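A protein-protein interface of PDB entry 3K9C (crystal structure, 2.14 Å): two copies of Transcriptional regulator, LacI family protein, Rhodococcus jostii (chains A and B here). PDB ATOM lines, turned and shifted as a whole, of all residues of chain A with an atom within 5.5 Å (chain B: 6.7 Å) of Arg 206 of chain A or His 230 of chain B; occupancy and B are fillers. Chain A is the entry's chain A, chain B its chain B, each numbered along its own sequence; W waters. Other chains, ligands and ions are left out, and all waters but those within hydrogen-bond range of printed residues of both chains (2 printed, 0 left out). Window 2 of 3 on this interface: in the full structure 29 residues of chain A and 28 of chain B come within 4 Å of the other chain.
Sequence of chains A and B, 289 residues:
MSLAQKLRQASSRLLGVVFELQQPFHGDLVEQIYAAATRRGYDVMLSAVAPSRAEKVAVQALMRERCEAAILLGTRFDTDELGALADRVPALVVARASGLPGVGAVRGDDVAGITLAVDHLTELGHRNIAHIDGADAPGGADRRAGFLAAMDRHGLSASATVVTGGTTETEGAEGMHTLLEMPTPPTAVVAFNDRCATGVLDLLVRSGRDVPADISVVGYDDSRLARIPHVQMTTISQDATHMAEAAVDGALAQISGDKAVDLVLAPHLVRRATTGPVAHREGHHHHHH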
ATOM      1  N   GLU A 169      -3.602  23.023  17.219  1.00  0.00           N
ATOM      2  CA  GLU A 169      -2.370  22.567  16.594  1.00  0.00           C
ATOM      3  C   GLU A 169      -1.987  23.384  15.368  1.00  0.00           C
ATOM      4  O   GLU A 169      -0.800  23.594  15.106  1.00  0.00           O
ATOM      5  CB  GLU A 169      -2.492  21.095  16.194  1.00  0.00           C
ATOM      6  CG  GLU A 169      -2.886  20.178  17.327  1.00  0.00           C
ATOM      7  CD  GLU A 169      -4.368  19.839  17.322  1.00  0.00           C
ATOM      8  OE1 GLU A 169      -5.199  20.761  17.164  1.00  0.00           O
ATOM      9  OE2 GLU A 169      -4.693  18.641  17.483  1.00  0.00           O
ATOM     10  N   THR A 170      -2.981  23.838  14.613  1.00  0.00           N
ATOM     11  CA  THR A 170      -2.707  24.616  13.409  1.00  0.00           C
ATOM     12  C   THR A 170      -2.038  25.943  13.747  1.00  0.00           C
ATOM     13  O   THR A 170      -1.050  26.329  13.126  1.00  0.00           O
ATOM     14  CB  THR A 170      -4.002  24.897  12.612  1.00  0.00           C
ATOM     15  OG1 THR A 170      -4.630  23.657  12.267  1.00  0.00           O
ATOM     16  CG2 THR A 170      -3.681  25.659  11.327  1.00  0.00           C
ATOM     17  N   ALA A 173       1.466  25.323  14.490  1.00  0.00           N
ATOM     18  CA  ALA A 173       2.230  25.078  13.271  1.00  0.00           C
ATOM     19  C   ALA A 173       2.453  26.343  12.447  1.00  0.00           C
ATOM     20  O   ALA A 173       3.540  26.559  11.913  1.00  0.00           O
ATOM     21  CB  ALA A 173       1.525  24.026  12.428  1.00  0.00           C
ATOM     22  N   THR A 198       2.129  20.769  20.046  1.00  0.00           N
ATOM     23  CA  THR A 198       2.086  19.575  19.211  1.00  0.00           C
ATOM     24  C   THR A 198       2.247  20.037  17.760  1.00  0.00           C
ATOM     25  O   THR A 198       3.048  19.478  17.001  1.00  0.00           O
ATOM     26  CB  THR A 198       0.754  18.819  19.362  1.00  0.00           C
ATOM     27  OG1 THR A 198       0.625  18.342  20.706  1.00  0.00           O
ATOM     28  CG2 THR A 198       0.713  17.635  18.418  1.00  0.00           C
ATOM     29  N   GLY A 199       1.501  21.078  17.393  1.00  0.00           N
ATOM     30  CA  GLY A 199       1.580  21.613  16.044  1.00  0.00           C
ATOM     31  C   GLY A 199       2.969  22.133  15.721  1.00  0.00           C
ATOM     32  O   GLY A 199       3.445  22.001  14.593  1.00  0.00           O
ATOM     33  N   LEU A 201       5.829  21.059  17.074  1.00  0.00           N
ATOM     34  CA  LEU A 201       6.665  19.875  16.895  1.00  0.00           C
ATOM     35  C   LEU A 201       6.447  19.215  15.539  1.00  0.00           C
ATOM     36  O   LEU A 201       7.406  18.856  14.862  1.00  0.00           O
ATOM     37  CB  LEU A 201       6.379  18.845  17.991  1.00  0.00           C
ATOM     38  CG  LEU A 201       6.798  19.214  19.412  1.00  0.00           C
ATOM     39  CD1 LEU A 201       6.372  18.094  20.352  1.00  0.00           C
ATOM     40  CD2 LEU A 201       8.314  19.436  19.468  1.00  0.00           C
ATOM     41  N   ASP A 202       5.182  19.052  15.156  1.00  0.00           N
ATOM     42  CA  ASP A 202       4.847  18.421  13.884  1.00  0.00           C
ATOM     43  C   ASP A 202       5.516  19.153  12.730  1.00  0.00           C
ATOM     44  O   ASP A 202       6.081  18.526  11.836  1.00  0.00           O
ATOM     45  CB  ASP A 202       3.329  18.399  13.663  1.00  0.00           C
ATOM     46  CG  ASP A 202       2.570  17.724  14.804  1.00  0.00           C
ATOM     47  OD1 ASP A 202       3.127  16.803  15.451  1.00  0.00           O
ATOM     48  OD2 ASP A 202       1.401  18.113  15.044  1.00  0.00           O
ATOM     49  N   LEU A 203       5.460  20.479  12.756  1.00  0.00           N
ATOM     50  CA  LEU A 203       6.060  21.269  11.695  1.00  0.00           C
ATOM     51  C   LEU A 203       7.573  21.130  11.672  1.00  0.00           C
ATOM     52  O   LEU A 203       8.165  20.971  10.605  1.00  0.00           O
ATOM     53  CB  LEU A 203       5.678  22.746  11.842  1.00  0.00           C
ATOM     54  CG  LEU A 203       6.255  23.670  10.757  1.00  0.00           C
ATOM     55  CD1 LEU A 203       5.408  24.914  10.626  1.00  0.00           C
ATOM     56  CD2 LEU A 203       7.688  24.043  11.101  1.00  0.00           C
ATOM     57  N   LEU A 204       8.202  21.184  12.842  1.00  0.00           N
ATOM     58  CA  LEU A 204       9.652  21.078  12.911  1.00  0.00           C
ATOM     59  C   LEU A 204      10.203  19.762  12.378  1.00  0.00           C
ATOM     60  O   LEU A 204      11.168  19.769  11.615  1.00  0.00           O
ATOM     61  CB  LEU A 204      10.141  21.290  14.345  1.00  0.00           C
ATOM     62  CG  LEU A 204       9.994  22.700  14.934  1.00  0.00           C
ATOM     63  CD1 LEU A 204      10.630  22.734  16.322  1.00  0.00           C
ATOM     64  CD2 LEU A 204      10.661  23.721  14.027  1.00  0.00           C
ATOM     65  N   VAL A 205       9.616  18.637  12.782  1.00  0.00           N
ATOM     66  CA  VAL A 205      10.095  17.342  12.306  1.00  0.00           C
ATOM     67  C   VAL A 205       9.893  17.195  10.796  1.00  0.00           C
ATOM     68  O   VAL A 205      10.769  16.687  10.093  1.00  0.00           O
ATOM     69  CB  VAL A 205       9.405  16.152  13.034  1.00  0.00           C
ATOM     70  CG1 VAL A 205       9.876  16.087  14.477  1.00  0.00           C
ATOM     71  CG2 VAL A 205       7.884  16.294  12.974  1.00  0.00           C
ATOM     72  N   ARG A 206       8.749  17.650  10.297  1.00  0.00           N
ATOM     73  CA  ARG A 206       8.480  17.559   8.865  1.00  0.00           C
ATOM     74  C   ARG A 206       9.403  18.485   8.075  1.00  0.00           C
ATOM     75  O   ARG A 206       9.616  18.284   6.884  1.00  0.00           O
ATOM     76  CB  ARG A 206       7.021  17.910   8.557  1.00  0.00           C
ATOM     77  CG  ARG A 206       5.995  16.972   9.180  1.00  0.00           C
ATOM     78  CD  ARG A 206       4.573  17.353   8.768  1.00  0.00           C
ATOM     79  NE  ARG A 206       3.563  16.937   9.743  1.00  0.00           N
ATOM     80  CZ  ARG A 206       3.286  15.675  10.057  1.00  0.00           C
ATOM     81  NH1 ARG A 206       3.940  14.683   9.469  1.00  0.00           N
ATOM     82  NH2 ARG A 206       2.356  15.404  10.964  1.00  0.00           N
ATOM     83  N   SER A 207       9.955  19.492   8.743  1.00  0.00           N
ATOM     84  CA  SER A 207      10.841  20.447   8.086  1.00  0.00           C
ATOM     85  C   SER A 207      12.309  20.069   8.221  1.00  0.00           C
ATOM     86  O   SER A 207      13.186  20.855   7.874  1.00  0.00           O
ATOM     87  CB  SER A 207      10.640  21.845   8.668  1.00  0.00           C
ATOM     88  OG  SER A 207      11.113  21.899   9.999  1.00  0.00           O
ATOM     89  N   GLY A 208      12.573  18.877   8.745  1.00  0.00           N
ATOM     90  CA  GLY A 208      13.944  18.423   8.891  1.00  0.00           C
ATOM     91  C   GLY A 208      14.698  18.901  10.119  1.00  0.00           C
ATOM     92  O   GLY A 208      15.887  18.609  10.273  1.00  0.00           O
ATOM     93  N   LEU B 201       1.897   7.970  12.079  1.00  0.00           N
ATOM     94  CA  LEU B 201       2.469   9.072  11.307  1.00  0.00           C
ATOM     95  C   LEU B 201       3.614   9.734  12.066  1.00  0.00           C
ATOM     96  O   LEU B 201       4.615  10.115  11.461  1.00  0.00           O
ATOM     97  CB  LEU B 201       1.401  10.127  11.007  1.00  0.00           C
ATOM     98  CG  LEU B 201       0.267   9.722  10.068  1.00  0.00           C
ATOM     99  CD1 LEU B 201      -0.814  10.797  10.081  1.00  0.00           C
ATOM    100  CD2 LEU B 201       0.812   9.514   8.665  1.00  0.00           C
ATOM    101  N   ASP B 202       3.450   9.888  13.383  1.00  0.00           N
ATOM    102  CA  ASP B 202       4.479  10.505  14.221  1.00  0.00           C
ATOM    103  C   ASP B 202       5.776   9.714  14.159  1.00  0.00           C
ATOM    104  O   ASP B 202       6.863  10.290  14.078  1.00  0.00           O
ATOM    105  CB  ASP B 202       4.056  10.568  15.688  1.00  0.00           C
ATOM    106  CG  ASP B 202       2.819  11.396  15.914  1.00  0.00           C
ATOM    107  OD1 ASP B 202       2.594  12.373  15.165  1.00  0.00           O
ATOM    108  OD2 ASP B 202       2.078  11.072  16.872  1.00  0.00           O
ATOM    109  N   VAL B 205       7.370   9.795  10.368  1.00  0.00           N
ATOM    110  CA  VAL B 205       8.038  11.040  10.019  1.00  0.00           C
ATOM    111  C   VAL B 205       9.329  11.200  10.819  1.00  0.00           C
ATOM    112  O   VAL B 205      10.314  11.715  10.308  1.00  0.00           O
ATOM    113  CB  VAL B 205       7.111  12.265  10.245  1.00  0.00           C
ATOM    114  CG1 VAL B 205       6.825  12.450  11.712  1.00  0.00           C
ATOM    115  CG2 VAL B 205       7.753  13.514   9.666  1.00  0.00           C
ATOM    116  N   ARG B 227      -8.730  15.825  10.153  1.00  0.00           N
ATOM    117  CA  ARG B 227      -8.935  17.007   9.332  1.00  0.00           C
ATOM    118  C   ARG B 227      -7.931  18.132   9.590  1.00  0.00           C
ATOM    119  O   ARG B 227      -7.863  19.091   8.820  1.00  0.00           O
ATOM    120  CB  ARG B 227     -10.362  17.523   9.515  1.00  0.00           C
ATOM    121  CG  ARG B 227     -10.574  18.322  10.783  1.00  0.00           C
ATOM    122  CD  ARG B 227     -12.055  18.508  11.094  1.00  0.00           C
ATOM    123  NE  ARG B 227     -12.663  17.243  11.504  1.00  0.00           N
ATOM    124  CZ  ARG B 227     -13.795  17.150  12.190  1.00  0.00           C
ATOM    125  NH1 ARG B 227     -14.442  18.254  12.540  1.00  0.00           N
ATOM    126  NH2 ARG B 227     -14.270  15.960  12.539  1.00  0.00           N
ATOM    127  N   ILE B 228      -7.154  18.020  10.664  1.00  0.00           N
ATOM    128  CA  ILE B 228      -6.162  19.041  10.970  1.00  0.00           C
ATOM    129  C   ILE B 228      -5.375  19.329   9.701  1.00  0.00           C
ATOM    130  O   ILE B 228      -4.832  18.421   9.084  1.00  0.00           O
ATOM    131  CB  ILE B 228      -5.186  18.584  12.079  1.00  0.00           C
ATOM    132  CG1 ILE B 228      -5.948  18.406  13.395  1.00  0.00           C
ATOM    133  CG2 ILE B 228      -4.079  19.611  12.248  1.00  0.00           C
ATOM    134  CD1 ILE B 228      -5.121  17.809  14.518  1.00  0.00           C
ATOM    135  N   PRO B 229      -5.313  20.607   9.295  1.00  0.00           N
ATOM    136  CA  PRO B 229      -4.618  21.095   8.106  1.00  0.00           C
ATOM    137  C   PRO B 229      -3.265  20.486   7.749  1.00  0.00           C
ATOM    138  O   PRO B 229      -3.009  20.226   6.574  1.00  0.00           O
ATOM    139  CB  PRO B 229      -4.528  22.593   8.363  1.00  0.00           C
ATOM    140  CG  PRO B 229      -5.823  22.867   9.013  1.00  0.00           C
ATOM    141  CD  PRO B 229      -5.937  21.733  10.015  1.00  0.00           C
ATOM    142  N   HIS B 230      -2.393  20.265   8.729  1.00  0.00           N
ATOM    143  CA  HIS B 230      -1.085  19.696   8.407  1.00  0.00           C
ATOM    144  C   HIS B 230      -1.014  18.180   8.561  1.00  0.00           C
ATOM    145  O   HIS B 230       0.021  17.572   8.292  1.00  0.00           O
ATOM    146  CB  HIS B 230       0.021  20.371   9.235  1.00  0.00           C
ATOM    147  CG  HIS B 230      -0.142  20.217  10.712  1.00  0.00           C
ATOM    148  ND1 HIS B 230       0.435  19.188  11.423  1.00  0.00           N
ATOM    149  CD2 HIS B 230      -0.844  20.949  11.613  1.00  0.00           C
ATOM    150  CE1 HIS B 230       0.095  19.288  12.696  1.00  0.00           C
ATOM    151  NE2 HIS B 230      -0.680  20.348  12.836  1.00  0.00           N
ATOM    152  N   VAL B 231      -2.115  17.569   8.988  1.00  0.00           N
ATOM    153  CA  VAL B 231      -2.148  16.120   9.136  1.00  0.00           C
ATOM    154  C   VAL B 231      -2.742  15.514   7.864  1.00  0.00           C
ATOM    155  O   VAL B 231      -2.132  14.640   7.246  1.00  0.00           O
ATOM    156  CB  VAL B 231      -2.983  15.697  10.366  1.00  0.00           C
ATOM    157  CG1 VAL B 231      -3.030  14.184  10.469  1.00  0.00           C
ATOM    158  CG2 VAL B 231      -2.370  16.285  11.628  1.00  0.00           C
ATOM    159  N   GLN B 232      -3.918  16.010   7.470  1.00  0.00           N
ATOM    160  CA  GLN B 232      -4.626  15.564   6.263  1.00  0.00           C
ATOM    161  C   GLN B 232      -4.637  14.039   6.117  1.00  0.00           C
ATOM    162  O   GLN B 232      -4.166  13.486   5.126  1.00  0.00           O
ATOM    163  CB  GLN B 232      -4.013  16.214   5.015  1.00  0.00           C
ATOM    164  CG  GLN B 232      -2.721  16.994   5.266  1.00  0.00           C
ATOM    165  CD  GLN B 232      -2.085  17.516   3.984  1.00  0.00           C
ATOM    166  OE1 GLN B 232      -2.700  18.282   3.230  1.00  0.00           O
ATOM    167  NE2 GLN B 232      -0.849  17.100   3.731  1.00  0.00           N
ATOM    168  N   MET B 233      -5.225  13.381   7.108  1.00  0.00           N
ATOM    169  CA  MET B 233      -5.300  11.929   7.163  1.00  0.00           C
ATOM    170  C   MET B 233      -6.454  11.272   6.403  1.00  0.00           C
ATOM    171  O   MET B 233      -7.625  11.620   6.588  1.00  0.00           O
ATOM    172  CB  MET B 233      -5.365  11.522   8.633  1.00  0.00           C
ATOM    173  CG  MET B 233      -5.191  10.057   8.924  1.00  0.00           C
ATOM    174  SD  MET B 233      -5.693   9.856  10.772  1.00  0.00           S
ATOM    175  CE  MET B 233      -4.054  10.529  11.545  1.00  0.00           C
HETATM  176  O   HOH W   1       0.842  13.517   8.572  1.00  0.00           O
HETATM  177  O   HOH W   2       4.325  14.513  14.099  1.00  0.00           O
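Positions printed for both chains: 201, 202 and 205.
Among the printed residues, merely in contact across the chains: Glu 169 of chain A with Ile 228 of chain B, Glu 169 of chain A with His 230 of chain B, Thr 170 of chain A with Pro 229 of chain B, Ala 173 of chain A with His 230 of chain B, Asp 202 of chain A with His 230 of chain B, Arg 206 of chain A with Val 205 of chain B and Arg 206 of chain A with His 230 of chain B.
Along chain A the printed residues that touch a printed residue of chain B span positions 169 to 206. Printed residues of chain B that touch a printed residue of chain A: Val 205, Ile 228, Pro 229 and His 230. Hydrophobic or aromatic side chains of chain B within 4 Å of the printed part of chain A: Val 205, Ile 228, Pro 229 and His 230. Among the printed residues, 7 pairs touch across the chains. Among the printed residues, no Asp or Glu carboxylate lies within 4 Å of a Lys or Arg side-chain nitrogen of the other chain.
Water W2 bridges OD1 of Asp 202 of chain A (2.9 Å) and OD1 of Asp 202 of chain B (3.0 Å). Water W1 lies within hydrogen-bond range of the guanidinium group of Arg 206 of chain A (3.4 Å) and the backbone carbonyl oxygen of Val 231 of chain B (3.4 Å).
Of the printed residues of chain B, Thr 170 of chain A touches Pro 229. Printed residues of chain B within 4 Å of Ala 173 of chain A: His 230 (3.97 Å). Leu 203 of chain A touches none of the printed residues of chain B. Printed residues of chain B within 4 Å of Arg 206 of chain A: Val 205 and His 230. Gly 208 of chain A touches none of the printed residues of chain B. Of the printed residues of chain A, Val 205 of chain B touches Arg 206. Printed residues of chain A within 4 Å of Ile 228 of chain B: Glu 169 (3.1 Å). Printed residues of chain A within 4 Å of Pro 229 of chain B: Thr 170. The nearest residue of chain B that does not touch Arg 206 of chain A is Val 231 of chain B (4.9 Å).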
